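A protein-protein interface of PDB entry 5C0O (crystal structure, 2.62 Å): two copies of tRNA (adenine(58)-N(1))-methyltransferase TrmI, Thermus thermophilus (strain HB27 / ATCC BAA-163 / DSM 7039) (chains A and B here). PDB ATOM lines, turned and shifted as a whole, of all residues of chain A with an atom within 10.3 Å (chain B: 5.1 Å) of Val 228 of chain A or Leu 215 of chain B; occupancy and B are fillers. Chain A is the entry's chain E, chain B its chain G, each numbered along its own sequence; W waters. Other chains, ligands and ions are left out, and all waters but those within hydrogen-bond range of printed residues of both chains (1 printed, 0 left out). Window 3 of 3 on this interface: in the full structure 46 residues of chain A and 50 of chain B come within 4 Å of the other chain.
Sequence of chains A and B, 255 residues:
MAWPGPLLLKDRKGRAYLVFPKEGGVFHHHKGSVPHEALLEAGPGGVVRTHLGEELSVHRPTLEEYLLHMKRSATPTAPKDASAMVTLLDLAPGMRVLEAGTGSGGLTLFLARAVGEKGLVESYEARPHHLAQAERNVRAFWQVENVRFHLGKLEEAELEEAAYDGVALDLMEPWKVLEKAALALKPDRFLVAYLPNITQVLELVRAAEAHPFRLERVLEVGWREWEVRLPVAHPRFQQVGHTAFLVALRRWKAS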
ATOM      1  N   LYS A  10     -26.207 -21.222   2.207  1.00  0.00           N
ATOM      2  CA  LYS A  10     -25.248 -22.270   2.543  1.00  0.00           C
ATOM      3  C   LYS A  10     -25.208 -22.524   4.050  1.00  0.00           C
ATOM      4  O   LYS A  10     -25.362 -21.599   4.847  1.00  0.00           O
ATOM      5  CB  LYS A  10     -23.851 -21.899   2.037  1.00  0.00           C
ATOM      6  CG  LYS A  10     -23.843 -21.209   0.677  1.00  0.00           C
ATOM      7  CD  LYS A  10     -22.723 -21.708  -0.217  1.00  0.00           C
ATOM      8  CE  LYS A  10     -21.350 -21.490   0.395  1.00  0.00           C
ATOM      9  NZ  LYS A  10     -21.164 -20.105   0.907  1.00  0.00           N
ATOM     10  N   GLY A  14     -21.335 -26.543   3.975  1.00  0.00           N
ATOM     11  CA  GLY A  14     -20.991 -25.991   2.678  1.00  0.00           C
ATOM     12  C   GLY A  14     -22.009 -26.329   1.604  1.00  0.00           C
ATOM     13  O   GLY A  14     -21.896 -25.867   0.469  1.00  0.00           O
ATOM     14  N   SER A  57     -25.976 -18.733   5.769  1.00  0.00           N
ATOM     15  CA  SER A  57     -25.486 -17.501   5.152  1.00  0.00           C
ATOM     16  C   SER A  57     -26.089 -17.294   3.765  1.00  0.00           C
ATOM     17  O   SER A  57     -26.226 -18.235   2.987  1.00  0.00           O
ATOM     18  CB  SER A  57     -23.957 -17.516   5.069  1.00  0.00           C
ATOM     19  OG  SER A  57     -23.489 -18.610   4.300  1.00  0.00           O
ATOM     20  N   HIS A  59     -26.527 -15.134   0.009  1.00  0.00           N
ATOM     21  CA  HIS A  59     -25.652 -14.591  -1.033  1.00  0.00           C
ATOM     22  C   HIS A  59     -26.367 -14.184  -2.320  1.00  0.00           C
ATOM     23  O   HIS A  59     -27.425 -14.716  -2.656  1.00  0.00           O
ATOM     24  CB  HIS A  59     -24.582 -15.618  -1.419  1.00  0.00           C
ATOM     25  CG  HIS A  59     -23.925 -16.289  -0.255  1.00  0.00           C
ATOM     26  ND1 HIS A  59     -22.843 -15.748   0.404  1.00  0.00           N
ATOM     27  CD2 HIS A  59     -24.187 -17.468   0.355  1.00  0.00           C
ATOM     28  CE1 HIS A  59     -22.472 -16.561   1.376  1.00  0.00           C
ATOM     29  NE2 HIS A  59     -23.271 -17.613   1.367  1.00  0.00           N
ATOM     30  N   GLU A  65     -21.954 -20.330  -9.280  1.00  0.00           N
ATOM     31  CA  GLU A  65     -22.875 -20.933  -8.321  1.00  0.00           C
ATOM     32  C   GLU A  65     -24.229 -21.211  -8.959  1.00  0.00           C
ATOM     33  O   GLU A  65     -24.869 -22.222  -8.666  1.00  0.00           O
ATOM     34  CB  GLU A  65     -23.043 -20.023  -7.102  1.00  0.00           C
ATOM     35  CG  GLU A  65     -21.865 -20.078  -6.129  1.00  0.00           C
ATOM     36  CD  GLU A  65     -21.699 -18.813  -5.295  1.00  0.00           C
ATOM     37  OE1 GLU A  65     -22.364 -17.797  -5.589  1.00  0.00           O
ATOM     38  OE2 GLU A  65     -20.894 -18.840  -4.339  1.00  0.00           O
ATOM     39  N   ARG A 224      -8.139 -27.111  -9.971  1.00  0.00           N
ATOM     40  CA  ARG A 224      -7.757 -28.054  -8.934  1.00  0.00           C
ATOM     41  C   ARG A 224      -7.847 -27.365  -7.568  1.00  0.00           C
ATOM     42  O   ARG A 224      -7.062 -26.475  -7.245  1.00  0.00           O
ATOM     43  CB  ARG A 224      -6.362 -28.614  -9.275  1.00  0.00           C
ATOM     44  CG  ARG A 224      -5.278 -28.655  -8.204  1.00  0.00           C
ATOM     45  CD  ARG A 224      -5.397 -29.864  -7.302  1.00  0.00           C
ATOM     46  NE  ARG A 224      -4.073 -30.386  -6.969  1.00  0.00           N
ATOM     47  CZ  ARG A 224      -3.811 -31.659  -6.692  1.00  0.00           C
ATOM     48  NH1 ARG A 224      -4.781 -32.565  -6.699  1.00  0.00           N
ATOM     49  NH2 ARG A 224      -2.571 -32.031  -6.407  1.00  0.00           N
ATOM     50  N   GLU A 225      -8.859 -27.761  -6.799  1.00  0.00           N
ATOM     51  CA  GLU A 225      -9.206 -27.104  -5.539  1.00  0.00           C
ATOM     52  C   GLU A 225      -8.404 -27.622  -4.349  1.00  0.00           C
ATOM     53  O   GLU A 225      -7.917 -28.754  -4.360  1.00  0.00           O
ATOM     54  CB  GLU A 225     -10.697 -27.294  -5.239  1.00  0.00           C
ATOM     55  CG  GLU A 225     -11.648 -26.959  -6.389  1.00  0.00           C
ATOM     56  CD  GLU A 225     -11.928 -25.472  -6.533  1.00  0.00           C
ATOM     57  OE1 GLU A 225     -11.635 -24.702  -5.594  1.00  0.00           O
ATOM     58  OE2 GLU A 225     -12.450 -25.074  -7.595  1.00  0.00           O
ATOM     59  N   TRP A 226      -8.288 -26.782  -3.323  1.00  0.00           N
ATOM     60  CA  TRP A 226      -7.715 -27.182  -2.041  1.00  0.00           C
ATOM     61  C   TRP A 226      -8.742 -27.070  -0.932  1.00  0.00           C
ATOM     62  O   TRP A 226      -9.823 -26.508  -1.117  1.00  0.00           O
ATOM     63  CB  TRP A 226      -6.506 -26.317  -1.681  1.00  0.00           C
ATOM     64  CG  TRP A 226      -5.295 -26.600  -2.485  1.00  0.00           C
ATOM     65  CD1 TRP A 226      -5.209 -26.643  -3.839  1.00  0.00           C
ATOM     66  CD2 TRP A 226      -3.980 -26.869  -1.987  1.00  0.00           C
ATOM     67  NE1 TRP A 226      -3.924 -26.927  -4.222  1.00  0.00           N
ATOM     68  CE2 TRP A 226      -3.148 -27.070  -3.103  1.00  0.00           C
ATOM     69  CE3 TRP A 226      -3.426 -26.959  -0.707  1.00  0.00           C
ATOM     70  CZ2 TRP A 226      -1.791 -27.358  -2.980  1.00  0.00           C
ATOM     71  CZ3 TRP A 226      -2.077 -27.245  -0.587  1.00  0.00           C
ATOM     72  CH2 TRP A 226      -1.276 -27.441  -1.717  1.00  0.00           C
ATOM     73  N   GLU A 227      -8.384 -27.617   0.222  1.00  0.00           N
ATOM     74  CA  GLU A 227      -9.085 -27.338   1.460  1.00  0.00           C
ATOM     75  C   GLU A 227      -8.096 -26.667   2.391  1.00  0.00           C
ATOM     76  O   GLU A 227      -7.054 -27.242   2.703  1.00  0.00           O
ATOM     77  CB  GLU A 227      -9.637 -28.612   2.097  1.00  0.00           C
ATOM     78  CG  GLU A 227     -10.949 -28.396   2.829  1.00  0.00           C
ATOM     79  CD  GLU A 227     -11.302 -29.541   3.758  1.00  0.00           C
ATOM     80  OE1 GLU A 227     -12.357 -29.460   4.421  1.00  0.00           O
ATOM     81  OE2 GLU A 227     -10.527 -30.518   3.831  1.00  0.00           O
ATOM     82  N   VAL A 228      -8.405 -25.444   2.808  1.00  0.00           N
ATOM     83  CA  VAL A 228      -7.603 -24.768   3.815  1.00  0.00           C
ATOM     84  C   VAL A 228      -8.480 -24.420   5.005  1.00  0.00           C
ATOM     85  O   VAL A 228      -9.224 -23.439   4.992  1.00  0.00           O
ATOM     86  CB  VAL A 228      -6.929 -23.496   3.277  1.00  0.00           C
ATOM     87  CG1 VAL A 228      -6.076 -22.854   4.369  1.00  0.00           C
ATOM     88  CG2 VAL A 228      -6.070 -23.826   2.067  1.00  0.00           C
ATOM     89  N   ARG A 229      -8.395 -25.267   6.021  1.00  0.00           N
ATOM     90  CA  ARG A 229      -8.974 -24.999   7.321  1.00  0.00           C
ATOM     91  C   ARG A 229      -7.824 -25.038   8.307  1.00  0.00           C
ATOM     92  O   ARG A 229      -7.809 -25.881   9.202  1.00  0.00           O
ATOM     93  CB  ARG A 229     -10.053 -26.025   7.678  1.00  0.00           C
ATOM     94  N   LEU A 230      -6.860 -24.137   8.104  1.00  0.00           N
ATOM     95  CA  LEU A 230      -5.614 -24.097   8.873  1.00  0.00           C
ATOM     96  C   LEU A 230      -5.838 -24.512  10.322  1.00  0.00           C
ATOM     97  O   LEU A 230      -6.729 -23.977  10.984  1.00  0.00           O
ATOM     98  CB  LEU A 230      -4.997 -22.691   8.841  1.00  0.00           C
ATOM     99  CG  LEU A 230      -4.345 -22.183   7.550  1.00  0.00           C
ATOM    100  CD1 LEU A 230      -3.878 -20.746   7.740  1.00  0.00           C
ATOM    101  CD2 LEU A 230      -3.178 -23.057   7.119  1.00  0.00           C
ATOM    102  N   PRO A 231      -5.024 -25.450  10.835  1.00  0.00           N
ATOM    103  CA  PRO A 231      -3.814 -26.074  10.269  1.00  0.00           C
ATOM    104  C   PRO A 231      -3.966 -27.130   9.149  1.00  0.00           C
ATOM    105  O   PRO A 231      -2.920 -27.623   8.721  1.00  0.00           O
ATOM    106  CB  PRO A 231      -3.166 -26.737  11.496  1.00  0.00           C
ATOM    107  CG  PRO A 231      -4.253 -26.875  12.498  1.00  0.00           C
ATOM    108  CD  PRO A 231      -5.160 -25.723  12.276  1.00  0.00           C
ATOM    109  N   VAL A 232      -5.164 -27.478   8.677  1.00  0.00           N
ATOM    110  CA  VAL A 232      -5.245 -28.402   7.536  1.00  0.00           C
ATOM    111  C   VAL A 232      -5.147 -27.579   6.253  1.00  0.00           C
ATOM    112  O   VAL A 232      -5.747 -26.509   6.137  1.00  0.00           O
ATOM    113  CB  VAL A 232      -6.545 -29.296   7.520  1.00  0.00           C
ATOM    114  CG1 VAL A 232      -7.306 -29.232   8.840  1.00  0.00           C
ATOM    115  CG2 VAL A 232      -7.470 -28.970   6.327  1.00  0.00           C
ATOM    116  N   ALA A 233      -4.365 -28.079   5.302  1.00  0.00           N
ATOM    117  CA  ALA A 233      -4.107 -27.374   4.053  1.00  0.00           C
ATOM    118  C   ALA A 233      -3.681 -28.362   2.976  1.00  0.00           C
ATOM    119  O   ALA A 233      -2.526 -28.781   2.941  1.00  0.00           O
ATOM    120  CB  ALA A 233      -3.036 -26.321   4.252  1.00  0.00           C
ATOM    121  N   HIS A 234      -4.607 -28.747   2.103  1.00  0.00           N
ATOM    122  CA  HIS A 234      -4.283 -29.715   1.061  1.00  0.00           C
ATOM    123  C   HIS A 234      -5.251 -29.669  -0.120  1.00  0.00           C
ATOM    124  O   HIS A 234      -6.370 -29.174   0.008  1.00  0.00           O
ATOM    125  CB  HIS A 234      -4.269 -31.130   1.646  1.00  0.00           C
ATOM    126  CG  HIS A 234      -5.612 -31.613   2.101  1.00  0.00           C
ATOM    127  ND1 HIS A 234      -6.586 -32.035   1.223  1.00  0.00           N
ATOM    128  CD2 HIS A 234      -6.142 -31.743   3.340  1.00  0.00           C
ATOM    129  CE1 HIS A 234      -7.658 -32.405   1.900  1.00  0.00           C
ATOM    130  NE2 HIS A 234      -7.416 -32.237   3.187  1.00  0.00           N
ATOM    131  N   PRO A 235      -4.811 -30.181  -1.283  1.00  0.00           N
ATOM    132  CA  PRO A 235      -5.716 -30.393  -2.417  1.00  0.00           C
ATOM    133  C   PRO A 235      -6.862 -31.320  -2.027  1.00  0.00           C
ATOM    134  O   PRO A 235      -6.627 -32.294  -1.317  1.00  0.00           O
ATOM    135  CB  PRO A 235      -4.814 -31.036  -3.475  1.00  0.00           C
ATOM    136  CG  PRO A 235      -3.442 -30.607  -3.120  1.00  0.00           C
ATOM    137  CD  PRO A 235      -3.416 -30.506  -1.629  1.00  0.00           C
ATOM    138  N   ARG A 236      -8.077 -31.023  -2.474  1.00  0.00           N
ATOM    139  CA  ARG A 236      -9.237 -31.821  -2.092  1.00  0.00           C
ATOM    140  C   ARG A 236      -9.061 -33.287  -2.478  1.00  0.00           C
ATOM    141  O   ARG A 236      -8.564 -33.598  -3.559  1.00  0.00           O
ATOM    142  CB  ARG A 236     -10.508 -31.261  -2.731  1.00  0.00           C
ATOM    143  CG  ARG A 236     -11.058 -30.019  -2.045  1.00  0.00           C
ATOM    144  CD  ARG A 236     -12.563 -30.131  -1.871  1.00  0.00           C
ATOM    145  NE  ARG A 236     -13.181 -28.871  -1.473  1.00  0.00           N
ATOM    146  CZ  ARG A 236     -14.432 -28.758  -1.038  1.00  0.00           C
ATOM    147  NH1 ARG A 236     -15.202 -29.834  -0.930  1.00  0.00           N
ATOM    148  NH2 ARG A 236     -14.915 -27.570  -0.702  1.00  0.00           N
ATOM    149  N   PHE A 237      -9.465 -34.178  -1.575  1.00  0.00           N
ATOM    150  CA  PHE A 237      -9.360 -35.617  -1.796  1.00  0.00           C
ATOM    151  C   PHE A 237     -10.196 -36.050  -2.991  1.00  0.00           C
ATOM    152  O   PHE A 237      -9.674 -36.594  -3.966  1.00  0.00           O
ATOM    153  CB  PHE A 237      -9.812 -36.385  -0.550  1.00  0.00           C
ATOM    154  CG  PHE A 237      -8.970 -36.125   0.667  1.00  0.00           C
ATOM    155  CD1 PHE A 237      -7.594 -36.004   0.566  1.00  0.00           C
ATOM    156  CD2 PHE A 237      -9.558 -36.003   1.915  1.00  0.00           C
ATOM    157  CE1 PHE A 237      -6.821 -35.767   1.685  1.00  0.00           C
ATOM    158  CE2 PHE A 237      -8.789 -35.764   3.038  1.00  0.00           C
ATOM    159  CZ  PHE A 237      -7.419 -35.647   2.922  1.00  0.00           C
ATOM    160  N   VAL B 205      -4.380 -16.209   4.155  1.00  0.00           N
ATOM    161  CA  VAL B 205      -5.481 -16.871   4.849  1.00  0.00           C
ATOM    162  C   VAL B 205      -5.362 -16.608   6.349  1.00  0.00           C
ATOM    163  O   VAL B 205      -6.368 -16.518   7.055  1.00  0.00           O
ATOM    164  CB  VAL B 205      -5.501 -18.400   4.595  1.00  0.00           C
ATOM    165  CG1 VAL B 205      -6.678 -19.054   5.313  1.00  0.00           C
ATOM    166  CG2 VAL B 205      -5.581 -18.702   3.106  1.00  0.00           C
ATOM    167  N   PHE B 213     -13.561 -11.454   6.319  1.00  0.00           N
ATOM    168  CA  PHE B 213     -13.492 -12.334   5.157  1.00  0.00           C
ATOM    169  C   PHE B 213     -13.668 -13.819   5.475  1.00  0.00           C
ATOM    170  O   PHE B 213     -13.065 -14.365   6.399  1.00  0.00           O
ATOM    171  CB  PHE B 213     -12.165 -12.117   4.426  1.00  0.00           C
ATOM    172  CG  PHE B 213     -12.127 -10.849   3.621  1.00  0.00           C
ATOM    173  CD1 PHE B 213     -13.046 -10.639   2.607  1.00  0.00           C
ATOM    174  CD2 PHE B 213     -11.184  -9.869   3.876  1.00  0.00           C
ATOM    175  CE1 PHE B 213     -13.030  -9.479   1.865  1.00  0.00           C
ATOM    176  CE2 PHE B 213     -11.160  -8.702   3.132  1.00  0.00           C
ATOM    177  CZ  PHE B 213     -12.085  -8.509   2.125  1.00  0.00           C
ATOM    178  N   ARG B 214     -14.507 -14.447   4.657  1.00  0.00           N
ATOM    179  CA  ARG B 214     -14.811 -15.872   4.717  1.00  0.00           C
ATOM    180  C   ARG B 214     -14.179 -16.553   3.508  1.00  0.00           C
ATOM    181  O   ARG B 214     -14.697 -16.449   2.397  1.00  0.00           O
ATOM    182  CB  ARG B 214     -16.332 -16.100   4.730  1.00  0.00           C
ATOM    183  CG  ARG B 214     -17.100 -14.985   4.017  1.00  0.00           C
ATOM    184  CD  ARG B 214     -18.561 -15.285   3.696  1.00  0.00           C
ATOM    185  NE  ARG B 214     -19.320 -15.877   4.799  1.00  0.00           N
ATOM    186  CZ  ARG B 214     -20.015 -15.195   5.709  1.00  0.00           C
ATOM    187  NH1 ARG B 214     -20.050 -13.866   5.695  1.00  0.00           N
ATOM    188  NH2 ARG B 214     -20.675 -15.853   6.653  1.00  0.00           N
ATOM    189  N   LEU B 215     -13.058 -17.237   3.723  1.00  0.00           N
ATOM    190  CA  LEU B 215     -12.318 -17.870   2.631  1.00  0.00           C
ATOM    191  C   LEU B 215     -13.150 -18.928   1.923  1.00  0.00           C
ATOM    192  O   LEU B 215     -13.614 -19.887   2.536  1.00  0.00           O
ATOM    193  CB  LEU B 215     -11.015 -18.480   3.158  1.00  0.00           C
ATOM    194  CG  LEU B 215     -10.233 -19.426   2.238  1.00  0.00           C
ATOM    195  CD1 LEU B 215      -9.419 -18.657   1.198  1.00  0.00           C
ATOM    196  CD2 LEU B 215      -9.340 -20.322   3.069  1.00  0.00           C
ATOM    197  N   GLU B 216     -13.319 -18.734   0.618  1.00  0.00           N
ATOM    198  CA  GLU B 216     -14.145 -19.609  -0.202  1.00  0.00           C
ATOM    199  C   GLU B 216     -13.317 -20.593  -1.025  1.00  0.00           C
ATOM    200  O   GLU B 216     -13.634 -21.783  -1.067  1.00  0.00           O
ATOM    201  CB  GLU B 216     -15.019 -18.769  -1.137  1.00  0.00           C
ATOM    202  CG  GLU B 216     -16.088 -17.942  -0.425  1.00  0.00           C
ATOM    203  CD  GLU B 216     -17.467 -18.596  -0.400  1.00  0.00           C
ATOM    204  OE1 GLU B 216     -17.651 -19.669  -1.013  1.00  0.00           O
ATOM    205  OE2 GLU B 216     -18.375 -18.023   0.237  1.00  0.00           O
ATOM    206  N   ARG B 217     -12.265 -20.103  -1.680  1.00  0.00           N
ATOM    207  CA  ARG B 217     -11.538 -20.916  -2.656  1.00  0.00           C
ATOM    208  C   ARG B 217     -10.017 -20.766  -2.603  1.00  0.00           C
ATOM    209  O   ARG B 217      -9.482 -19.676  -2.389  1.00  0.00           O
ATOM    210  CB  ARG B 217     -12.006 -20.577  -4.077  1.00  0.00           C
ATOM    211  CG  ARG B 217     -13.514 -20.637  -4.294  1.00  0.00           C
ATOM    212  CD  ARG B 217     -13.982 -22.030  -4.663  1.00  0.00           C
ATOM    213  NE  ARG B 217     -13.668 -22.353  -6.051  1.00  0.00           N
ATOM    214  CZ  ARG B 217     -14.354 -21.903  -7.097  1.00  0.00           C
ATOM    215  NH1 ARG B 217     -15.398 -21.105  -6.918  1.00  0.00           N
ATOM    216  NH2 ARG B 217     -13.995 -22.248  -8.325  1.00  0.00           N
ATOM    217  N   VAL B 218      -9.344 -21.895  -2.806  1.00  0.00           N
ATOM    218  CA  VAL B 218      -7.915 -21.951  -3.090  1.00  0.00           C
ATOM    219  C   VAL B 218      -7.748 -22.964  -4.213  1.00  0.00           C
ATOM    220  O   VAL B 218      -7.965 -24.155  -3.993  1.00  0.00           O
ATOM    221  CB  VAL B 218      -7.079 -22.391  -1.870  1.00  0.00           C
ATOM    222  CG1 VAL B 218      -5.594 -22.439  -2.224  1.00  0.00           C
ATOM    223  CG2 VAL B 218      -7.322 -21.478  -0.680  1.00  0.00           C
ATOM    224  N   VAL B 247      -6.605 -17.175  -4.876  1.00  0.00           N
ATOM    225  CA  VAL B 247      -7.237 -17.112  -3.560  1.00  0.00           C
ATOM    226  C   VAL B 247      -8.471 -16.220  -3.579  1.00  0.00           C
ATOM    227  O   VAL B 247      -8.340 -15.011  -3.721  1.00  0.00           O
ATOM    228  CB  VAL B 247      -6.277 -16.555  -2.489  1.00  0.00           C
ATOM    229  CG1 VAL B 247      -6.899 -16.703  -1.099  1.00  0.00           C
ATOM    230  CG2 VAL B 247      -4.904 -17.226  -2.567  1.00  0.00           C
ATOM    231  N   ALA B 248      -9.652 -16.807  -3.396  1.00  0.00           N
ATOM    232  CA  ALA B 248     -10.902 -16.043  -3.400  1.00  0.00           C
ATOM    233  C   ALA B 248     -11.441 -15.837  -1.983  1.00  0.00           C
ATOM    234  O   ALA B 248     -11.713 -16.800  -1.265  1.00  0.00           O
ATOM    235  CB  ALA B 248     -11.940 -16.741  -4.258  1.00  0.00           C
ATOM    236  N   LEU B 249     -11.600 -14.570  -1.600  1.00  0.00           N
ATOM    237  CA  LEU B 249     -12.065 -14.196  -0.261  1.00  0.00           C
ATOM    238  C   LEU B 249     -13.336 -13.345  -0.314  1.00  0.00           C
ATOM    239  O   LEU B 249     -13.284 -12.172  -0.682  1.00  0.00           O
ATOM    240  CB  LEU B 249     -10.962 -13.432   0.484  1.00  0.00           C
ATOM    241  CG  LEU B 249      -9.866 -14.283   1.135  1.00  0.00           C
ATOM    242  CD1 LEU B 249      -8.648 -13.456   1.501  1.00  0.00           C
ATOM    243  CD2 LEU B 249     -10.410 -14.962   2.370  1.00  0.00           C
HETATM  244  O   HOH W   1     -11.314 -24.339  -2.931  1.00  0.00           O
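No position is printed for both chains.
The backbone carbonyl oxygen of Lys 10 of chain A is in hydrogen-bond range of the backbone NH of Ser 57 of chain A, at 3.1 Å. The side-chain amino group (NZ) of Lys 10 of chain A is in hydrogen-bond range of a ring nitrogen (NE2) of His 59 of chain A (3.3 Å). The backbone carbonyl oxygen (O) of Glu 225 of chain A sits at hydrogen-bond distance from the backbone NH (N) of Arg 236 of chain A (3.0 Å). O of Ala 248 of chain B sits at hydrogen-bond distance from N of Glu 216 of chain B, at 3.1 Å. N of Ala 248 of chain B sits at hydrogen-bond distance from O of Arg 217 of chain B, at 3.0 Å.
The side-chain carboxylate (OE2) of Glu 216 of chain B is in salt-bridge range of the side-chain amino group (NZ) of Lys 10 of chain A (3.5 Å). OE1 of Glu 225 of chain A is in salt-bridge range of NE of Arg 217 of chain B (3.1 Å). O of Val 218 of chain B lies within hydrogen-bond range of N of Trp 226 of chain A.
Among the printed residues, merely in contact across the chains: Glu 225 of chain A with Val 218 of chain B (3.5 Å), Val 228 of chain A with Leu 215 of chain B (3.7 Å), Val 228 of chain A with Val 218 of chain B (3.8 Å) and Val 228 of chain A with Val 205 of chain B (3.96 Å).
Val 228 of chain A touches three residues of chain B. Leu 215 of chain B touches just one residue of chain A: Val 228 (3.7 Å). Of the printed residues of chain B, Glu 225 of chain A touches Arg 217 (3.1 Å) and Val 218 (3.5 Å). Of the printed residues of chain B, Trp 226 of chain A touches Val 218. Printed residues of chain A within 4 Å of Val 205 of chain B: Val 228. Arg 214 of chain B touches none of the printed residues of chain A. Ala 233 of chain A touches none of the printed residues of chain B. The nearest residue of chain A that does not touch Leu 215 of chain B is Arg 229 of chain A (5.8 Å).
Water W1 lies within hydrogen-bond range of the side-chain carboxylate (OE1) of Glu 225 of chain A, the backbone NH (N) of Val 218 of chain B and the backbone carbonyl oxygen (O) of Trp 226 of chain A.
Printed residues of chain B that touch a printed residue of chain A: Val 205, Leu 215, Glu 216, Arg 217 and Val 218. Hydrophobic or aromatic side chains of chain B that line the printed part of chain A: Val 205, Leu 215 and Val 218. Hydrophobic or aromatic side chains of chain A within 4 Å of the printed part of chain B: Trp 226 and Val 228. Among the printed residues, Asp or Glu carboxylates within 4 Å of a Lys or Arg side-chain nitrogen of the other chain: Lys 10 of chain A with Glu 216 of chain B and Glu 225 of chain A with Arg 217 of chain B.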
